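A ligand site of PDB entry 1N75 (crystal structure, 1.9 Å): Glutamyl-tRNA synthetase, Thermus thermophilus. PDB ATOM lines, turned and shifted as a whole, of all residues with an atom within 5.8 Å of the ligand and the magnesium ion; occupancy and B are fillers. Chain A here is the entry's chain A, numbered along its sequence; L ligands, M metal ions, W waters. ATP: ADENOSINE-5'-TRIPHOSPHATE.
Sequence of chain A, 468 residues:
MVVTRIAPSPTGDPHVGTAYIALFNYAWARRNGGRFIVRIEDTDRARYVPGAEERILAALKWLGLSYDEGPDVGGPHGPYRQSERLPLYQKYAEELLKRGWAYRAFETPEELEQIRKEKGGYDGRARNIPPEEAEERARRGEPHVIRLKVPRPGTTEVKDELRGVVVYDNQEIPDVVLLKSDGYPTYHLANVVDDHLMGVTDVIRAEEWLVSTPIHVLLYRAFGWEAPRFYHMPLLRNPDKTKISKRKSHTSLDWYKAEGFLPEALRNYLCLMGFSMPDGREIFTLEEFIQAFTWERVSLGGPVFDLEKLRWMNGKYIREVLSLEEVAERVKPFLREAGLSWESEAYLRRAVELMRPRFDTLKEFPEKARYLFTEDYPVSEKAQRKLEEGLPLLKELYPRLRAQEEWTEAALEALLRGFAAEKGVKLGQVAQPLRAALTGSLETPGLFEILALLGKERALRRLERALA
The side-chain hydroxyl of Ser 245 sits at hydrogen-bond distance from an oxygen (O2G) of the ligand, at 2.5 Å. The guanidinium group (NE) of Arg 247 is in salt-bridge range of an oxygen (O3G) of the ligand (2.6 Å). OE2 of Glu 208 sits at hydrogen-bond distance from O2' of the ligand (2.7 Å). O2B of the ligand sits at hydrogen-bond distance from N of Lys 246, at 2.8 Å. The side-chain amino group (NZ) of Lys 246 is in salt-bridge range of an oxygen (O2A) of the ligand, 3.0 Å away. The backbone NH of Leu 236 lies within hydrogen-bond range of a nitrogen (N1) of the ligand (2.9 Å). The backbone carbonyl oxygen of Leu 236 is in hydrogen-bond range of a nitrogen (N6) of the ligand. O2B of the ligand is in hydrogen-bond range of NE2 of His 15 (2.9 Å). O2B of the ligand lies within salt-bridge range of NZ of Lys 243 (3.9 Å). The backbone carbonyl oxygen of Ile 244 lies within hydrogen-bond range of a nitrogen (N6) of the ligand (3.1 Å).
N of Arg 247 sits close to OG of Ser 245 (3.2 Å). N of Ile 244 sits at hydrogen-bond distance from O of Leu 236 (2.9 Å). N of Gly 17 sits at hydrogen-bond distance from ND1 of His 15 (2.8 Å). The side-chain hydroxyl of Tyr 20 sits at hydrogen-bond distance from the backbone carbonyl oxygen of Pro 234 (2.7 Å).
Residues that only touch the ligand: Gly 17 (3.7 Å), Thr 18 (3.9 Å), Tyr 20 (3.96 Å), Ala 206 (3.7 Å), Trp 209 (3.6 Å) and Leu 235 (3.6 Å). Hydrophobic or aromatic side chains within 4 Å of the ligand: His 15, Tyr 20, Ala 206, Leu 235, Leu 236 and Ile 244. 14 residues have an atom within 4 Å of the ligand: His 15, Gly 17, Thr 18, Tyr 20, Ala 206, Glu 208, Trp 209, Leu 235, Leu 236, Lys 243, Ile 244, Ser 245, Lys 246 and Arg 247. The nearest printed residue that does not touch the ligand is Ile 21 (4.7 Å).
No residue comes within 4 Å of the magnesium ion.
The magnesium ion is bound by O1G of the ligand (2.0 Å), O1B of the ligand (2.0 Å), water W3 (2.0 Å), water W7 (2.1 Å), water W10 (2.1 Å) and O1A of the ligand (2.1 Å).
Water W7 lies within hydrogen-bond range of OE1 of Glu 208 (3.0 Å) and NZ of Lys 243 (3.3 Å). Water W10 bridges the side-chain carboxylate of Glu 208 (2.7 Å) and an oxygen (O5') of the ligand (3.3 Å). Water W9 bridges O2G of the ligand (2.5 Å) and NZ of Lys 243 (3.0 Å). Water W6 bridges an oxygen (O3') of the ligand (2.6 Å) and the indole nitrogen (NE1) of Trp 209 (3.4 Å). Water W1 bridges OG1 of Thr 18 (2.7 Å) and O3' of the ligand (2.8 Å). Water W4 lies within hydrogen-bond range of the backbone NH of Ala 206 (2.9 Å), the indole nitrogen of Trp 209 (3.4 Å) and an oxygen (O2') of the ligand (3.4 Å).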
ATOM      1  N   ALA A   7       8.664 -26.544   8.890  1.00  0.00           N
ATOM      2  CA  ALA A   7       9.951 -27.166   9.147  1.00  0.00           C
ATOM      3  C   ALA A   7      10.935 -26.095   9.570  1.00  0.00           C
ATOM      4  O   ALA A   7      11.823 -25.714   8.814  1.00  0.00           O
ATOM      5  CB  ALA A   7      10.446 -27.864   7.884  1.00  0.00           C
ATOM      6  N   THR A  11      18.017 -22.247  14.690  1.00  0.00           N
ATOM      7  CA  THR A  11      19.308 -21.603  14.554  1.00  0.00           C
ATOM      8  C   THR A  11      19.422 -20.252  15.245  1.00  0.00           C
ATOM      9  O   THR A  11      20.430 -19.566  15.103  1.00  0.00           O
ATOM     10  CB  THR A  11      19.642 -21.423  13.064  1.00  0.00           C
ATOM     11  OG1 THR A  11      18.583 -20.707  12.416  1.00  0.00           O
ATOM     12  CG2 THR A  11      19.784 -22.776  12.398  1.00  0.00           C
ATOM     13  N   HIS A  15      11.566 -16.879  14.473  1.00  0.00           N
ATOM     14  CA  HIS A  15      11.366 -15.858  13.444  1.00  0.00           C
ATOM     15  C   HIS A  15       9.886 -15.592  13.143  1.00  0.00           C
ATOM     16  O   HIS A  15       9.062 -16.497  13.108  1.00  0.00           O
ATOM     17  CB  HIS A  15      12.100 -16.309  12.177  1.00  0.00           C
ATOM     18  CG  HIS A  15      12.473 -15.206  11.240  1.00  0.00           C
ATOM     19  ND1 HIS A  15      11.539 -14.500  10.504  1.00  0.00           N
ATOM     20  CD2 HIS A  15      13.688 -14.726  10.866  1.00  0.00           C
ATOM     21  CE1 HIS A  15      12.166 -13.652   9.709  1.00  0.00           C
ATOM     22  NE2 HIS A  15      13.467 -13.772   9.901  1.00  0.00           N
ATOM     23  N   GLY A  17       8.764 -14.804  10.393  1.00  0.00           N
ATOM     24  CA  GLY A  17       8.463 -15.415   9.113  1.00  0.00           C
ATOM     25  C   GLY A  17       7.960 -16.839   9.319  1.00  0.00           C
ATOM     26  O   GLY A  17       7.149 -17.355   8.539  1.00  0.00           O
ATOM     27  N   THR A  18       8.456 -17.474  10.379  1.00  0.00           N
ATOM     28  CA  THR A  18       8.046 -18.836  10.701  1.00  0.00           C
ATOM     29  C   THR A  18       6.600 -18.828  11.199  1.00  0.00           C
ATOM     30  O   THR A  18       5.826 -19.728  10.886  1.00  0.00           O
ATOM     31  CB  THR A  18       8.974 -19.447  11.782  1.00  0.00           C
ATOM     32  OG1 THR A  18      10.308 -19.501  11.275  1.00  0.00           O
ATOM     33  CG2 THR A  18       8.522 -20.847  12.159  1.00  0.00           C
ATOM     34  N   TYR A  20       4.345 -16.635  10.418  1.00  0.00           N
ATOM     35  CA  TYR A  20       3.574 -16.287   9.230  1.00  0.00           C
ATOM     36  C   TYR A  20       3.281 -17.546   8.404  1.00  0.00           C
ATOM     37  O   TYR A  20       2.122 -17.831   8.073  1.00  0.00           O
ATOM     38  CB  TYR A  20       4.367 -15.252   8.425  1.00  0.00           C
ATOM     39  CG  TYR A  20       3.922 -14.991   6.998  1.00  0.00           C
ATOM     40  CD1 TYR A  20       2.628 -14.556   6.704  1.00  0.00           C
ATOM     41  CD2 TYR A  20       4.833 -15.123   5.952  1.00  0.00           C
ATOM     42  CE1 TYR A  20       2.264 -14.249   5.381  1.00  0.00           C
ATOM     43  CE2 TYR A  20       4.484 -14.821   4.645  1.00  0.00           C
ATOM     44  CZ  TYR A  20       3.200 -14.379   4.364  1.00  0.00           C
ATOM     45  OH  TYR A  20       2.870 -14.041   3.069  1.00  0.00           O
ATOM     46  N   ILE A  21       4.328 -18.307   8.109  1.00  0.00           N
ATOM     47  CA  ILE A  21       4.170 -19.516   7.329  1.00  0.00           C
ATOM     48  C   ILE A  21       3.364 -20.557   8.099  1.00  0.00           C
ATOM     49  O   ILE A  21       2.518 -21.252   7.514  1.00  0.00           O
ATOM     50  CB  ILE A  21       5.547 -20.102   6.917  1.00  0.00           C
ATOM     51  CG1 ILE A  21       6.262 -19.135   5.980  1.00  0.00           C
ATOM     52  CG2 ILE A  21       5.358 -21.459   6.247  1.00  0.00           C
ATOM     53  CD1 ILE A  21       5.477 -18.782   4.704  1.00  0.00           C
ATOM     54  N   ALA A 206       7.662 -20.220   2.132  1.00  0.00           N
ATOM     55  CA  ALA A 206       8.011 -18.890   1.627  1.00  0.00           C
ATOM     56  C   ALA A 206       8.402 -18.930   0.144  1.00  0.00           C
ATOM     57  O   ALA A 206       9.040 -19.880  -0.308  1.00  0.00           O
ATOM     58  CB  ALA A 206       9.140 -18.301   2.454  1.00  0.00           C
ATOM     59  N   GLU A 208      10.711 -17.650  -1.447  1.00  0.00           N
ATOM     60  CA  GLU A 208      12.131 -17.724  -1.768  1.00  0.00           C
ATOM     61  C   GLU A 208      12.551 -19.160  -2.123  1.00  0.00           C
ATOM     62  O   GLU A 208      13.671 -19.386  -2.594  1.00  0.00           O
ATOM     63  CB  GLU A 208      12.978 -17.158  -0.615  1.00  0.00           C
ATOM     64  CG  GLU A 208      12.803 -17.823   0.739  1.00  0.00           C
ATOM     65  CD  GLU A 208      13.549 -17.076   1.845  1.00  0.00           C
ATOM     66  OE1 GLU A 208      14.418 -16.237   1.511  1.00  0.00           O
ATOM     67  OE2 GLU A 208      13.294 -17.344   3.042  1.00  0.00           O
ATOM     68  N   TRP A 209      11.657 -20.117  -1.901  1.00  0.00           N
ATOM     69  CA  TRP A 209      11.934 -21.516  -2.186  1.00  0.00           C
ATOM     70  C   TRP A 209      11.271 -21.953  -3.497  1.00  0.00           C
ATOM     71  O   TRP A 209      11.445 -23.084  -3.933  1.00  0.00           O
ATOM     72  CB  TRP A 209      11.411 -22.411  -1.052  1.00  0.00           C
ATOM     73  CG  TRP A 209      11.953 -22.039   0.291  1.00  0.00           C
ATOM     74  CD1 TRP A 209      11.229 -21.739   1.408  1.00  0.00           C
ATOM     75  CD2 TRP A 209      13.327 -21.879   0.646  1.00  0.00           C
ATOM     76  NE1 TRP A 209      12.064 -21.401   2.434  1.00  0.00           N
ATOM     77  CE2 TRP A 209      13.366 -21.476   2.003  1.00  0.00           C
ATOM     78  CE3 TRP A 209      14.545 -22.031  -0.044  1.00  0.00           C
ATOM     79  CZ2 TRP A 209      14.565 -21.217   2.684  1.00  0.00           C
ATOM     80  CZ3 TRP A 209      15.735 -21.779   0.625  1.00  0.00           C
ATOM     81  CH2 TRP A 209      15.731 -21.372   1.979  1.00  0.00           C
ATOM     82  N   PRO A 234       3.939 -15.122  -0.480  1.00  0.00           N
ATOM     83  CA  PRO A 234       4.724 -13.918  -0.790  1.00  0.00           C
ATOM     84  C   PRO A 234       5.548 -13.545   0.438  1.00  0.00           C
ATOM     85  O   PRO A 234       5.074 -13.676   1.566  1.00  0.00           O
ATOM     86  CB  PRO A 234       3.651 -12.882  -1.107  1.00  0.00           C
ATOM     87  CG  PRO A 234       2.508 -13.710  -1.632  1.00  0.00           C
ATOM     88  CD  PRO A 234       2.505 -14.873  -0.672  1.00  0.00           C
ATOM     89  N   LEU A 235       6.771 -13.079   0.225  1.00  0.00           N
ATOM     90  CA  LEU A 235       7.629 -12.686   1.336  1.00  0.00           C
ATOM     91  C   LEU A 235       7.127 -11.424   2.028  1.00  0.00           C
ATOM     92  O   LEU A 235       6.553 -10.543   1.384  1.00  0.00           O
ATOM     93  CB  LEU A 235       9.065 -12.447   0.852  1.00  0.00           C
ATOM     94  CG  LEU A 235       9.876 -13.634   0.339  1.00  0.00           C
ATOM     95  CD1 LEU A 235      11.249 -13.154  -0.113  1.00  0.00           C
ATOM     96  CD2 LEU A 235      10.013 -14.676   1.435  1.00  0.00           C
ATOM     97  N   LEU A 236       7.350 -11.346   3.335  1.00  0.00           N
ATOM     98  CA  LEU A 236       6.971 -10.168   4.104  1.00  0.00           C
ATOM     99  C   LEU A 236       7.966  -9.076   3.711  1.00  0.00           C
ATOM    100  O   LEU A 236       9.171  -9.331   3.656  1.00  0.00           O
ATOM    101  CB  LEU A 236       7.087 -10.445   5.602  1.00  0.00           C
ATOM    102  CG  LEU A 236       6.202 -11.565   6.168  1.00  0.00           C
ATOM    103  CD1 LEU A 236       6.536 -11.799   7.622  1.00  0.00           C
ATOM    104  CD2 LEU A 236       4.732 -11.187   6.016  1.00  0.00           C
ATOM    105  N   ARG A 237       7.461  -7.872   3.454  1.00  0.00           N
ATOM    106  CA  ARG A 237       8.306  -6.761   3.035  1.00  0.00           C
ATOM    107  C   ARG A 237       8.325  -5.569   3.985  1.00  0.00           C
ATOM    108  O   ARG A 237       7.387  -5.343   4.741  1.00  0.00           O
ATOM    109  CB  ARG A 237       7.854  -6.245   1.655  1.00  0.00           C
ATOM    110  CG  ARG A 237       7.736  -7.297   0.578  1.00  0.00           C
ATOM    111  CD  ARG A 237       9.075  -7.924   0.242  1.00  0.00           C
ATOM    112  NE  ARG A 237       8.943  -8.908  -0.824  1.00  0.00           N
ATOM    113  CZ  ARG A 237       8.547  -8.622  -2.071  1.00  0.00           C
ATOM    114  NH1 ARG A 237       8.258  -7.375  -2.404  1.00  0.00           N
ATOM    115  NH2 ARG A 237       8.439  -9.595  -2.964  1.00  0.00           N
ATOM    116  N   LYS A 243      12.720  -7.093   1.235  1.00  0.00           N
ATOM    117  CA  LYS A 243      12.383  -8.259   2.032  1.00  0.00           C
ATOM    118  C   LYS A 243      12.769  -8.068   3.493  1.00  0.00           C
ATOM    119  O   LYS A 243      13.888  -7.664   3.800  1.00  0.00           O
ATOM    120  CB  LYS A 243      13.120  -9.485   1.469  1.00  0.00           C
ATOM    121  CG  LYS A 243      13.143 -10.678   2.388  1.00  0.00           C
ATOM    122  CD  LYS A 243      14.113 -11.739   1.889  1.00  0.00           C
ATOM    123  CE  LYS A 243      14.199 -12.879   2.874  1.00  0.00           C
ATOM    124  NZ  LYS A 243      14.649 -12.424   4.212  1.00  0.00           N
ATOM    125  N   ILE A 244      11.849  -8.355   4.408  1.00  0.00           N
ATOM    126  CA  ILE A 244      12.186  -8.221   5.827  1.00  0.00           C
ATOM    127  C   ILE A 244      13.278  -9.221   6.157  1.00  0.00           C
ATOM    128  O   ILE A 244      13.258 -10.361   5.694  1.00  0.00           O
ATOM    129  CB  ILE A 244      10.964  -8.480   6.713  1.00  0.00           C
ATOM    130  CG1 ILE A 244      10.015  -7.286   6.617  1.00  0.00           C
ATOM    131  CG2 ILE A 244      11.395  -8.694   8.162  1.00  0.00           C
ATOM    132  CD1 ILE A 244       8.851  -7.364   7.544  1.00  0.00           C
ATOM    133  N   SER A 245      14.253  -8.791   6.953  1.00  0.00           N
ATOM    134  CA  SER A 245      15.363  -9.640   7.346  1.00  0.00           C
ATOM    135  C   SER A 245      15.704  -9.444   8.814  1.00  0.00           C
ATOM    136  O   SER A 245      15.613  -8.330   9.351  1.00  0.00           O
ATOM    137  CB  SER A 245      16.595  -9.321   6.490  1.00  0.00           C
ATOM    138  OG  SER A 245      17.743 -10.003   6.973  1.00  0.00           O
ATOM    139  N   LYS A 246      16.100 -10.539   9.478  1.00  0.00           N
ATOM    140  CA  LYS A 246      16.450 -10.494  10.900  1.00  0.00           C
ATOM    141  C   LYS A 246      17.686  -9.633  11.114  1.00  0.00           C
ATOM    142  O   LYS A 246      17.966  -9.205  12.237  1.00  0.00           O
ATOM    143  CB  LYS A 246      16.723 -11.906  11.411  1.00  0.00           C
ATOM    144  CG  LYS A 246      17.946 -12.566  10.792  1.00  0.00           C
ATOM    145  CD  LYS A 246      18.059 -14.040  11.157  1.00  0.00           C
ATOM    146  CE  LYS A 246      19.269 -14.675  10.501  1.00  0.00           C
ATOM    147  NZ  LYS A 246      19.271 -16.163  10.686  1.00  0.00           N
ATOM    148  N   ARG A 247      18.429  -9.371  10.043  1.00  0.00           N
ATOM    149  CA  ARG A 247      19.644  -8.566  10.131  1.00  0.00           C
ATOM    150  C   ARG A 247      19.349  -7.084   9.921  1.00  0.00           C
ATOM    151  O   ARG A 247      20.223  -6.239  10.144  1.00  0.00           O
ATOM    152  CB  ARG A 247      20.661  -9.039   9.087  1.00  0.00           C
ATOM    153  CG  ARG A 247      21.030 -10.513   9.214  1.00  0.00           C
ATOM    154  CD  ARG A 247      21.877 -10.960   8.043  1.00  0.00           C
ATOM    155  NE  ARG A 247      22.116 -12.401   8.064  1.00  0.00           N
ATOM    156  CZ  ARG A 247      22.848 -13.030   8.984  1.00  0.00           C
ATOM    157  NH1 ARG A 247      23.429 -12.343   9.962  1.00  0.00           N
ATOM    158  NH2 ARG A 247      23.000 -14.346   8.925  1.00  0.00           N
ATOM    159  N   THR A 251      12.713  -9.319  14.017  1.00  0.00           N
ATOM    160  CA  THR A 251      11.965 -10.459  13.514  1.00  0.00           C
ATOM    161  C   THR A 251      11.740 -11.506  14.596  1.00  0.00           C
ATOM    162  O   THR A 251      10.991 -12.467  14.380  1.00  0.00           O
ATOM    163  CB  THR A 251      12.703 -11.123  12.353  1.00  0.00           C
ATOM    164  OG1 THR A 251      14.046 -11.416  12.741  1.00  0.00           O
ATOM    165  CG2 THR A 251      12.710 -10.202  11.134  1.00  0.00           C
HETATM  166  PG  ATP L   1      18.773 -13.531   6.426  1.00  0.00           P
HETATM  167  O1G ATP L   1      18.502 -14.521   5.307  1.00  0.00           O
HETATM  168  O2G ATP L   1      18.591 -12.107   5.920  1.00  0.00           O
HETATM  169  O3G ATP L   1      20.204 -13.696   6.913  1.00  0.00           O
HETATM  170  PB  ATP L   1      16.177 -14.047   7.458  1.00  0.00           P
HETATM  171  O1B ATP L   1      15.923 -14.452   6.047  1.00  0.00           O
HETATM  172  O2B ATP L   1      15.478 -12.866   8.026  1.00  0.00           O
HETATM  173  O3B ATP L   1      17.767 -13.811   7.671  1.00  0.00           O
HETATM  174  PA  ATP L   1      16.274 -16.835   8.038  1.00  0.00           P
HETATM  175  O1A ATP L   1      17.056 -16.775   6.778  1.00  0.00           O
HETATM  176  O2A ATP L   1      16.891 -17.406   9.264  1.00  0.00           O
HETATM  177  O3A ATP L   1      15.826 -15.315   8.429  1.00  0.00           O
HETATM  178  O5' ATP L   1      14.891 -17.583   7.779  1.00  0.00           O
HETATM  179  C5' ATP L   1      14.097 -18.050   8.865  1.00  0.00           C
HETATM  180  C4' ATP L   1      12.738 -18.467   8.372  1.00  0.00           C
HETATM  181  O4' ATP L   1      11.951 -17.275   8.084  1.00  0.00           O
HETATM  182  C3' ATP L   1      12.717 -19.299   7.093  1.00  0.00           C
HETATM  183  O3' ATP L   1      11.646 -20.237   7.134  1.00  0.00           O
HETATM  184  C2' ATP L   1      12.477 -18.254   6.008  1.00  0.00           C
HETATM  185  O2' ATP L   1      11.885 -18.767   4.842  1.00  0.00           O
HETATM  186  C1' ATP L   1      11.536 -17.288   6.724  1.00  0.00           C
HETATM  187  N9  ATP L   1      11.622 -15.912   6.229  1.00  0.00           N
HETATM  188  C8  ATP L   1      12.715 -15.097   6.227  1.00  0.00           C
HETATM  189  N7  ATP L   1      12.484 -13.899   5.739  1.00  0.00           N
HETATM  190  C5  ATP L   1      11.148 -13.935   5.394  1.00  0.00           C
HETATM  191  C6  ATP L   1      10.297 -12.973   4.837  1.00  0.00           C
HETATM  192  N6  ATP L   1      10.687 -11.731   4.520  1.00  0.00           N
HETATM  193  N1  ATP L   1       9.005 -13.330   4.599  1.00  0.00           N
HETATM  194  C2  ATP L   1       8.621 -14.574   4.928  1.00  0.00           C
HETATM  195  N3  ATP L   1       9.333 -15.564   5.478  1.00  0.00           N
HETATM  196  C4  ATP L   1      10.601 -15.177   5.685  1.00  0.00           C
HETATM  197 MG    MG M   1      16.973 -15.790   4.929  1.00  0.00          MG
HETATM  198  O   HOH W   1      10.910 -21.467   9.569  1.00  0.00           O
HETATM  199  O   HOH W   2      15.910 -17.984  11.667  1.00  0.00           O
HETATM  200  O   HOH W   3      18.232 -17.242   4.230  1.00  0.00           O
HETATM  201  O   HOH W   4       9.336 -21.033   4.358  1.00  0.00           O
HETATM  202  O   HOH W   5      21.055 -11.039   4.512  1.00  0.00           O
HETATM  203  O   HOH W   6      12.274 -22.308   5.677  1.00  0.00           O
HETATM  204  O   HOH W   7      16.552 -14.871   3.131  1.00  0.00           O
HETATM  205  O   HOH W   8      15.801 -19.765   5.462  1.00  0.00           O
HETATM  206  O   HOH W   9      17.482 -11.578   3.765  1.00  0.00           O
HETATM  207  O   HOH W  10      15.540 -17.249   4.566  1.00  0.00           O
